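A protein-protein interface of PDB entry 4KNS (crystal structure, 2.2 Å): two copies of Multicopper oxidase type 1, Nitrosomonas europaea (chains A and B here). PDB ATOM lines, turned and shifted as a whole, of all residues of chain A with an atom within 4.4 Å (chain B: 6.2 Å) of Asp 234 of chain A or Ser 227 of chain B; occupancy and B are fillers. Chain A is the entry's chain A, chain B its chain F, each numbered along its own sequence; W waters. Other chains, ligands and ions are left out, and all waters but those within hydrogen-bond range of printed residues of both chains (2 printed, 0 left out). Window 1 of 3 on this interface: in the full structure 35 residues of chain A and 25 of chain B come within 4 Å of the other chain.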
ATOM      1  N   VAL A 192      12.509  -3.852 -23.654  1.00  0.00           N
ATOM      2  CA  VAL A 192      11.232  -4.156 -24.289  1.00  0.00           C
ATOM      3  C   VAL A 192      11.180  -3.449 -25.642  1.00  0.00           C
ATOM      4  O   VAL A 192      11.522  -2.271 -25.744  1.00  0.00           O
ATOM      5  CB  VAL A 192      10.048  -3.677 -23.418  1.00  0.00           C
ATOM      6  CG1 VAL A 192       8.719  -3.877 -24.136  1.00  0.00           C
ATOM      7  CG2 VAL A 192      10.045  -4.390 -22.072  1.00  0.00           C
ATOM      8  N   ASN A 193      10.771  -4.172 -26.680  1.00  0.00           N
ATOM      9  CA  ASN A 193      10.477  -3.544 -27.964  1.00  0.00           C
ATOM     10  C   ASN A 193       8.967  -3.393 -28.150  1.00  0.00           C
ATOM     11  O   ASN A 193       8.272  -4.343 -28.526  1.00  0.00           O
ATOM     12  CB  ASN A 193      11.118  -4.317 -29.127  1.00  0.00           C
ATOM     13  CG  ASN A 193      10.972  -3.600 -30.466  1.00  0.00           C
ATOM     14  OD1 ASN A 193      10.514  -2.459 -30.538  1.00  0.00           O
ATOM     15  ND2 ASN A 193      11.366  -4.278 -31.538  1.00  0.00           N
ATOM     16  N   SER A 215      12.839 -13.324 -23.210  1.00  0.00           N
ATOM     17  CA  SER A 215      11.723 -13.098 -22.277  1.00  0.00           C
ATOM     18  C   SER A 215      12.155 -12.992 -20.808  1.00  0.00           C
ATOM     19  O   SER A 215      11.328 -13.102 -19.903  1.00  0.00           O
ATOM     20  CB  SER A 215      10.616 -14.145 -22.459  1.00  0.00           C
ATOM     21  OG  SER A 215       9.704 -13.747 -23.466  1.00  0.00           O
ATOM     22  N   ILE A 230      15.469  -8.371 -30.971  1.00  0.00           N
ATOM     23  CA  ILE A 230      14.209  -8.265 -30.244  1.00  0.00           C
ATOM     24  C   ILE A 230      13.146  -7.757 -31.210  1.00  0.00           C
ATOM     25  O   ILE A 230      13.183  -6.601 -31.642  1.00  0.00           O
ATOM     26  CB  ILE A 230      14.303  -7.343 -29.004  1.00  0.00           C
ATOM     27  CG1 ILE A 230      15.475  -7.735 -28.099  1.00  0.00           C
ATOM     28  CG2 ILE A 230      13.021  -7.401 -28.191  1.00  0.00           C
ATOM     29  CD1 ILE A 230      16.694  -6.849 -28.241  1.00  0.00           C
ATOM     30  N   GLY A 231      12.213  -8.638 -31.562  1.00  0.00           N
ATOM     31  CA  GLY A 231      11.129  -8.292 -32.481  1.00  0.00           C
ATOM     32  C   GLY A 231      10.094  -7.403 -31.823  1.00  0.00           C
ATOM     33  O   GLY A 231      10.131  -7.194 -30.606  1.00  0.00           O
ATOM     34  N   ALA A 232       9.178  -6.872 -32.629  1.00  0.00           N
ATOM     35  CA  ALA A 232       8.091  -6.043 -32.120  1.00  0.00           C
ATOM     36  C   ALA A 232       7.224  -6.852 -31.164  1.00  0.00           C
ATOM     37  O   ALA A 232       6.844  -7.983 -31.469  1.00  0.00           O
ATOM     38  CB  ALA A 232       7.257  -5.491 -33.266  1.00  0.00           C
ATOM     39  N   GLY A 233       6.939  -6.274 -30.000  1.00  0.00           N
ATOM     40  CA  GLY A 233       6.135  -6.935 -28.977  1.00  0.00           C
ATOM     41  C   GLY A 233       6.899  -7.953 -28.149  1.00  0.00           C
ATOM     42  O   GLY A 233       6.299  -8.731 -27.409  1.00  0.00           O
ATOM     43  N   ASP A 234       8.224  -7.953 -28.272  1.00  0.00           N
ATOM     44  CA  ASP A 234       9.060  -8.872 -27.508  1.00  0.00           C
ATOM     45  C   ASP A 234       9.885  -8.136 -26.454  1.00  0.00           C
ATOM     46  O   ASP A 234      10.020  -6.912 -26.505  1.00  0.00           O
ATOM     47  CB  ASP A 234       9.966  -9.684 -28.441  1.00  0.00           C
ATOM     48  CG  ASP A 234      10.449 -10.977 -27.808  1.00  0.00           C
ATOM     49  OD1 ASP A 234       9.877 -11.396 -26.775  1.00  0.00           O
ATOM     50  OD2 ASP A 234      11.399 -11.584 -28.345  1.00  0.00           O
ATOM     51  N   ALA A 235      10.422  -8.893 -25.498  1.00  0.00           N
ATOM     52  CA  ALA A 235      11.223  -8.341 -24.408  1.00  0.00           C
ATOM     53  C   ALA A 235      12.348  -9.295 -24.014  1.00  0.00           C
ATOM     54  O   ALA A 235      12.222 -10.508 -24.177  1.00  0.00           O
ATOM     55  CB  ALA A 235      10.339  -8.031 -23.207  1.00  0.00           C
ATOM     56  N   SER B 201       6.755 -11.782 -35.883  1.00  0.00           N
ATOM     57  CA  SER B 201       7.008 -11.757 -34.447  1.00  0.00           C
ATOM     58  C   SER B 201       5.794 -12.346 -33.725  1.00  0.00           C
ATOM     59  O   SER B 201       4.914 -11.616 -33.267  1.00  0.00           O
ATOM     60  CB  SER B 201       7.291 -10.323 -33.985  1.00  0.00           C
ATOM     61  OG  SER B 201       7.877 -10.300 -32.695  1.00  0.00           O
ATOM     62  N   LEU B 202       5.758 -13.673 -33.627  1.00  0.00           N
ATOM     63  CA  LEU B 202       4.550 -14.390 -33.217  1.00  0.00           C
ATOM     64  C   LEU B 202       4.303 -14.398 -31.707  1.00  0.00           C
ATOM     65  O   LEU B 202       5.146 -14.848 -30.928  1.00  0.00           O
ATOM     66  CB  LEU B 202       4.555 -15.817 -33.774  1.00  0.00           C
ATOM     67  CG  LEU B 202       3.180 -16.436 -34.049  1.00  0.00           C
ATOM     68  CD1 LEU B 202       2.495 -15.776 -35.242  1.00  0.00           C
ATOM     69  CD2 LEU B 202       3.300 -17.936 -34.263  1.00  0.00           C
ATOM     70  N   HIS B 203       3.125 -13.907 -31.319  1.00  0.00           N
ATOM     71  CA  HIS B 203       2.735 -13.777 -29.914  1.00  0.00           C
ATOM     72  C   HIS B 203       1.301 -14.198 -29.696  1.00  0.00           C
ATOM     73  O   HIS B 203       0.424 -13.856 -30.497  1.00  0.00           O
ATOM     74  CB  HIS B 203       2.958 -12.336 -29.447  1.00  0.00           C
ATOM     75  CG  HIS B 203       2.274 -11.992 -28.140  1.00  0.00           C
ATOM     76  ND1 HIS B 203       2.785 -12.329 -26.943  1.00  0.00           N
ATOM     77  CD2 HIS B 203       1.089 -11.303 -27.882  1.00  0.00           C
ATOM     78  CE1 HIS B 203       1.967 -11.891 -25.967  1.00  0.00           C
ATOM     79  NE2 HIS B 203       0.932 -11.261 -26.544  1.00  0.00           N
ATOM     80  N   PRO B 204       1.036 -14.956 -28.611  1.00  0.00           N
ATOM     81  CA  PRO B 204      -0.338 -15.281 -28.254  1.00  0.00           C
ATOM     82  C   PRO B 204      -0.904 -14.267 -27.255  1.00  0.00           C
ATOM     83  O   PRO B 204      -0.519 -14.269 -26.081  1.00  0.00           O
ATOM     84  CB  PRO B 204      -0.208 -16.669 -27.609  1.00  0.00           C
ATOM     85  CG  PRO B 204       1.219 -16.768 -27.147  1.00  0.00           C
ATOM     86  CD  PRO B 204       1.993 -15.597 -27.693  1.00  0.00           C
ATOM     87  N   TRP B 209       3.893 -18.626 -24.844  1.00  0.00           N
ATOM     88  CA  TRP B 209       4.395 -19.875 -25.415  1.00  0.00           C
ATOM     89  C   TRP B 209       5.027 -20.699 -24.332  1.00  0.00           C
ATOM     90  O   TRP B 209       6.022 -20.287 -23.735  1.00  0.00           O
ATOM     91  CB  TRP B 209       5.402 -19.619 -26.535  1.00  0.00           C
ATOM     92  CG  TRP B 209       4.881 -18.801 -27.694  1.00  0.00           C
ATOM     93  CD1 TRP B 209       5.398 -17.601 -28.183  1.00  0.00           C
ATOM     94  CD2 TRP B 209       3.726 -19.097 -28.558  1.00  0.00           C
ATOM     95  NE1 TRP B 209       4.666 -17.151 -29.251  1.00  0.00           N
ATOM     96  CE2 TRP B 209       3.650 -17.998 -29.530  1.00  0.00           C
ATOM     97  CE3 TRP B 209       2.783 -20.121 -28.621  1.00  0.00           C
ATOM     98  CZ2 TRP B 209       2.666 -17.948 -30.508  1.00  0.00           C
ATOM     99  CZ3 TRP B 209       1.796 -20.059 -29.613  1.00  0.00           C
ATOM    100  CH2 TRP B 209       1.740 -18.998 -30.532  1.00  0.00           C
ATOM    101  N   VAL B 212       9.067 -23.337 -27.161  1.00  0.00           N
ATOM    102  CA  VAL B 212       9.304 -23.032 -28.571  1.00  0.00           C
ATOM    103  C   VAL B 212      10.494 -23.853 -29.063  1.00  0.00           C
ATOM    104  O   VAL B 212      11.538 -23.901 -28.412  1.00  0.00           O
ATOM    105  CB  VAL B 212       9.551 -21.522 -28.816  1.00  0.00           C
ATOM    106  CG1 VAL B 212       9.867 -21.251 -30.282  1.00  0.00           C
ATOM    107  CG2 VAL B 212       8.345 -20.698 -28.388  1.00  0.00           C
ATOM    108  N   LEU B 225       8.277 -18.163 -23.686  1.00  0.00           N
ATOM    109  CA  LEU B 225       8.524 -16.984 -24.516  1.00  0.00           C
ATOM    110  C   LEU B 225       7.226 -16.246 -24.815  1.00  0.00           C
ATOM    111  O   LEU B 225       6.238 -16.862 -25.213  1.00  0.00           O
ATOM    112  CB  LEU B 225       9.215 -17.370 -25.831  1.00  0.00           C
ATOM    113  CG  LEU B 225      10.585 -18.060 -25.808  1.00  0.00           C
ATOM    114  CD1 LEU B 225      11.046 -18.323 -27.233  1.00  0.00           C
ATOM    115  CD2 LEU B 225      11.624 -17.242 -25.055  1.00  0.00           C
ATOM    116  N   GLN B 226       7.229 -14.929 -24.619  1.00  0.00           N
ATOM    117  CA  GLN B 226       6.057 -14.111 -24.943  1.00  0.00           C
ATOM    118  C   GLN B 226       5.913 -13.927 -26.456  1.00  0.00           C
ATOM    119  O   GLN B 226       4.799 -13.885 -26.980  1.00  0.00           O
ATOM    120  CB  GLN B 226       6.087 -12.765 -24.205  1.00  0.00           C
ATOM    121  CG  GLN B 226       7.134 -11.765 -24.670  1.00  0.00           C
ATOM    122  CD  GLN B 226       7.412 -10.702 -23.628  1.00  0.00           C
ATOM    123  OE1 GLN B 226       6.769  -9.649 -23.606  1.00  0.00           O
ATOM    124  NE2 GLN B 226       8.358 -10.982 -22.742  1.00  0.00           N
ATOM    125  N   SER B 227       7.047 -13.830 -27.143  1.00  0.00           N
ATOM    126  CA  SER B 227       7.079 -13.717 -28.595  1.00  0.00           C
ATOM    127  C   SER B 227       8.233 -14.536 -29.156  1.00  0.00           C
ATOM    128  O   SER B 227       9.168 -14.885 -28.431  1.00  0.00           O
ATOM    129  CB  SER B 227       7.219 -12.252 -29.024  1.00  0.00           C
ATOM    130  OG  SER B 227       6.114 -11.478 -28.594  1.00  0.00           O
ATOM    131  N   TYR B 228       8.163 -14.843 -30.448  1.00  0.00           N
ATOM    132  CA  TYR B 228       9.252 -15.527 -31.129  1.00  0.00           C
ATOM    133  C   TYR B 228       9.360 -15.077 -32.582  1.00  0.00           C
ATOM    134  O   TYR B 228       8.373 -15.099 -33.320  1.00  0.00           O
ATOM    135  CB  TYR B 228       9.089 -17.051 -31.033  1.00  0.00           C
ATOM    136  CG  TYR B 228      10.214 -17.819 -31.682  1.00  0.00           C
ATOM    137  CD1 TYR B 228      11.462 -17.922 -31.068  1.00  0.00           C
ATOM    138  CD2 TYR B 228      10.035 -18.434 -32.918  1.00  0.00           C
ATOM    139  CE1 TYR B 228      12.499 -18.619 -31.668  1.00  0.00           C
ATOM    140  CE2 TYR B 228      11.063 -19.134 -33.527  1.00  0.00           C
ATOM    141  CZ  TYR B 228      12.291 -19.224 -32.898  1.00  0.00           C
ATOM    142  OH  TYR B 228      13.308 -19.920 -33.508  1.00  0.00           O
ATOM    143  N   LEU B 229      10.565 -14.670 -32.978  1.00  0.00           N
ATOM    144  CA  LEU B 229      10.833 -14.222 -34.346  1.00  0.00           C
ATOM    145  C   LEU B 229      11.067 -15.374 -35.313  1.00  0.00           C
ATOM    146  O   LEU B 229      11.997 -16.169 -35.139  1.00  0.00           O
ATOM    147  CB  LEU B 229      12.043 -13.288 -34.389  1.00  0.00           C
ATOM    148  CG  LEU B 229      11.891 -11.828 -33.980  1.00  0.00           C
ATOM    149  CD1 LEU B 229      13.247 -11.149 -34.069  1.00  0.00           C
ATOM    150  CD2 LEU B 229      10.869 -11.114 -34.851  1.00  0.00           C
ATOM    151  N   LEU B 238       5.623 -24.260 -31.674  1.00  0.00           N
ATOM    152  CA  LEU B 238       5.297 -23.461 -30.498  1.00  0.00           C
ATOM    153  C   LEU B 238       4.111 -24.065 -29.745  1.00  0.00           C
ATOM    154  O   LEU B 238       3.071 -24.360 -30.340  1.00  0.00           O
ATOM    155  CB  LEU B 238       5.013 -22.001 -30.894  1.00  0.00           C
ATOM    156  CG  LEU B 238       6.047 -21.243 -31.743  1.00  0.00           C
ATOM    157  CD1 LEU B 238       5.804 -21.441 -33.233  1.00  0.00           C
ATOM    158  CD2 LEU B 238       6.046 -19.758 -31.416  1.00  0.00           C
ATOM    159  N   HIS B 253       3.167  -9.721 -34.106  1.00  0.00           N
ATOM    160  CA  HIS B 253       3.124  -8.542 -33.238  1.00  0.00           C
ATOM    161  C   HIS B 253       3.665  -7.280 -33.862  1.00  0.00           C
ATOM    162  O   HIS B 253       3.560  -6.202 -33.279  1.00  0.00           O
ATOM    163  CB  HIS B 253       3.789  -8.821 -31.893  1.00  0.00           C
ATOM    164  CG  HIS B 253       3.140  -8.100 -30.736  1.00  0.00           C
ATOM    165  ND1 HIS B 253       3.110  -6.759 -30.645  1.00  0.00           N
ATOM    166  CD2 HIS B 253       2.484  -8.585 -29.608  1.00  0.00           C
ATOM    167  CE1 HIS B 253       2.469  -6.401 -29.517  1.00  0.00           C
ATOM    168  NE2 HIS B 253       2.087  -7.519 -28.884  1.00  0.00           N
HETATM  169  O   HOH W   1      12.136 -14.825 -28.343  1.00  0.00           O
HETATM  170  O   HOH W   2      10.806 -13.759 -25.900  1.00  0.00           O
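OG of Ser 215 of chain A is in hydrogen-bond range of N of Gln 226 of chain B (3.0 Å).
O of Ala 232 of chain A sits at hydrogen-bond distance from OG of Ser 201 of chain B, 2.8 Å away.
OG of Ser 227 of chain B sits at hydrogen-bond distance from O of Gly 233 of chain A, at 3.0 Å.
The backbone carbonyl oxygen of Gln 226 of chain B is in hydrogen-bond range of a ring nitrogen (ND1) of His 203 of chain B (2.5 Å).
N of Asn 193 of chain A lies within hydrogen-bond range of O of Asp 234 of chain A, at 2.8 Å.
The backbone NH of Ser 215 of chain A is in hydrogen-bond range of the backbone carbonyl oxygen of Ala 235 of chain A (3.0 Å).
N of His 253 of chain B lies within hydrogen-bond range of O of Ser 201 of chain B.
O of Gly 231 of chain A lies within hydrogen-bond range of ND2 of Asn 193 of chain A (3.3 Å).
N of Gly 233 of chain A is in hydrogen-bond range of O of Asn 193 of chain A, at 2.8 Å.
Ser 215 of chain A touches Leu 225 of chain B (OG to CA, 3.6 Å).
Gly 231 of chain A touches Ser 201 of chain B.
Gly 231 of chain A touches Leu 229 of chain B (CA to CD2, 3.7 Å).
His 253 of chain B touches Ala 232 of chain A.
Gly 233 of chain A touches Gln 226 of chain B (O to OE1, 3.9 Å).
His 253 of chain B touches Gly 233 of chain A.
OD1 of Asp 234 of chain A touches CG of Gln 226 of chain B (3.5 Å).
CB of Ser 227 of chain B touches OD1 of Asp 234 of chain A (3.6 Å).
NE2 of Gln 226 of chain B touches CB of Ala 235 of chain A (3.6 Å).
Of chain B, only Gln 226 (3.5 Å) and Ser 227 (3.6 Å) come within 4 Å of Asp 234 of chain A.
Of chain A, only Gly 233 and Asp 234 come within 4 Å of Ser 227 of chain B.
Printed residues of chain A within 4 Å of Leu 229 of chain B: Gly 231.
Of the printed residues of chain B, Ala 235 of chain A touches Gln 226 (3.6 Å).
The nearest printed residue of chain A that does not touch Ser 227 of chain B is Ser 215 of chain A (4.5 Å).
The nearest printed residue of chain A that does not touch Ser 201 of chain B is Asp 234 of chain A (4.8 Å).
Hydrophobic or aromatic side chains of chain B that line the printed part of chain A: Leu 229 and His 253.
Hydrophobic or aromatic side chains of chain A within 4 Å of the printed part of chain B: Ala 232 and Ala 235.
Among the printed residues, no Asp or Glu carboxylate lies within 4 Å of a Lys or Arg side-chain nitrogen of the other chain.
No position is printed for both chains.
Water W2 lies within hydrogen-bond range of the side-chain hydroxyl of Ser 215 of chain A, the side-chain carboxylate of Asp 234 of chain A and the backbone carbonyl oxygen of Ser 227 of chain B.
Water W1 bridges O of Ser 227 of chain B and OD2 of Asp 234 of chain A.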
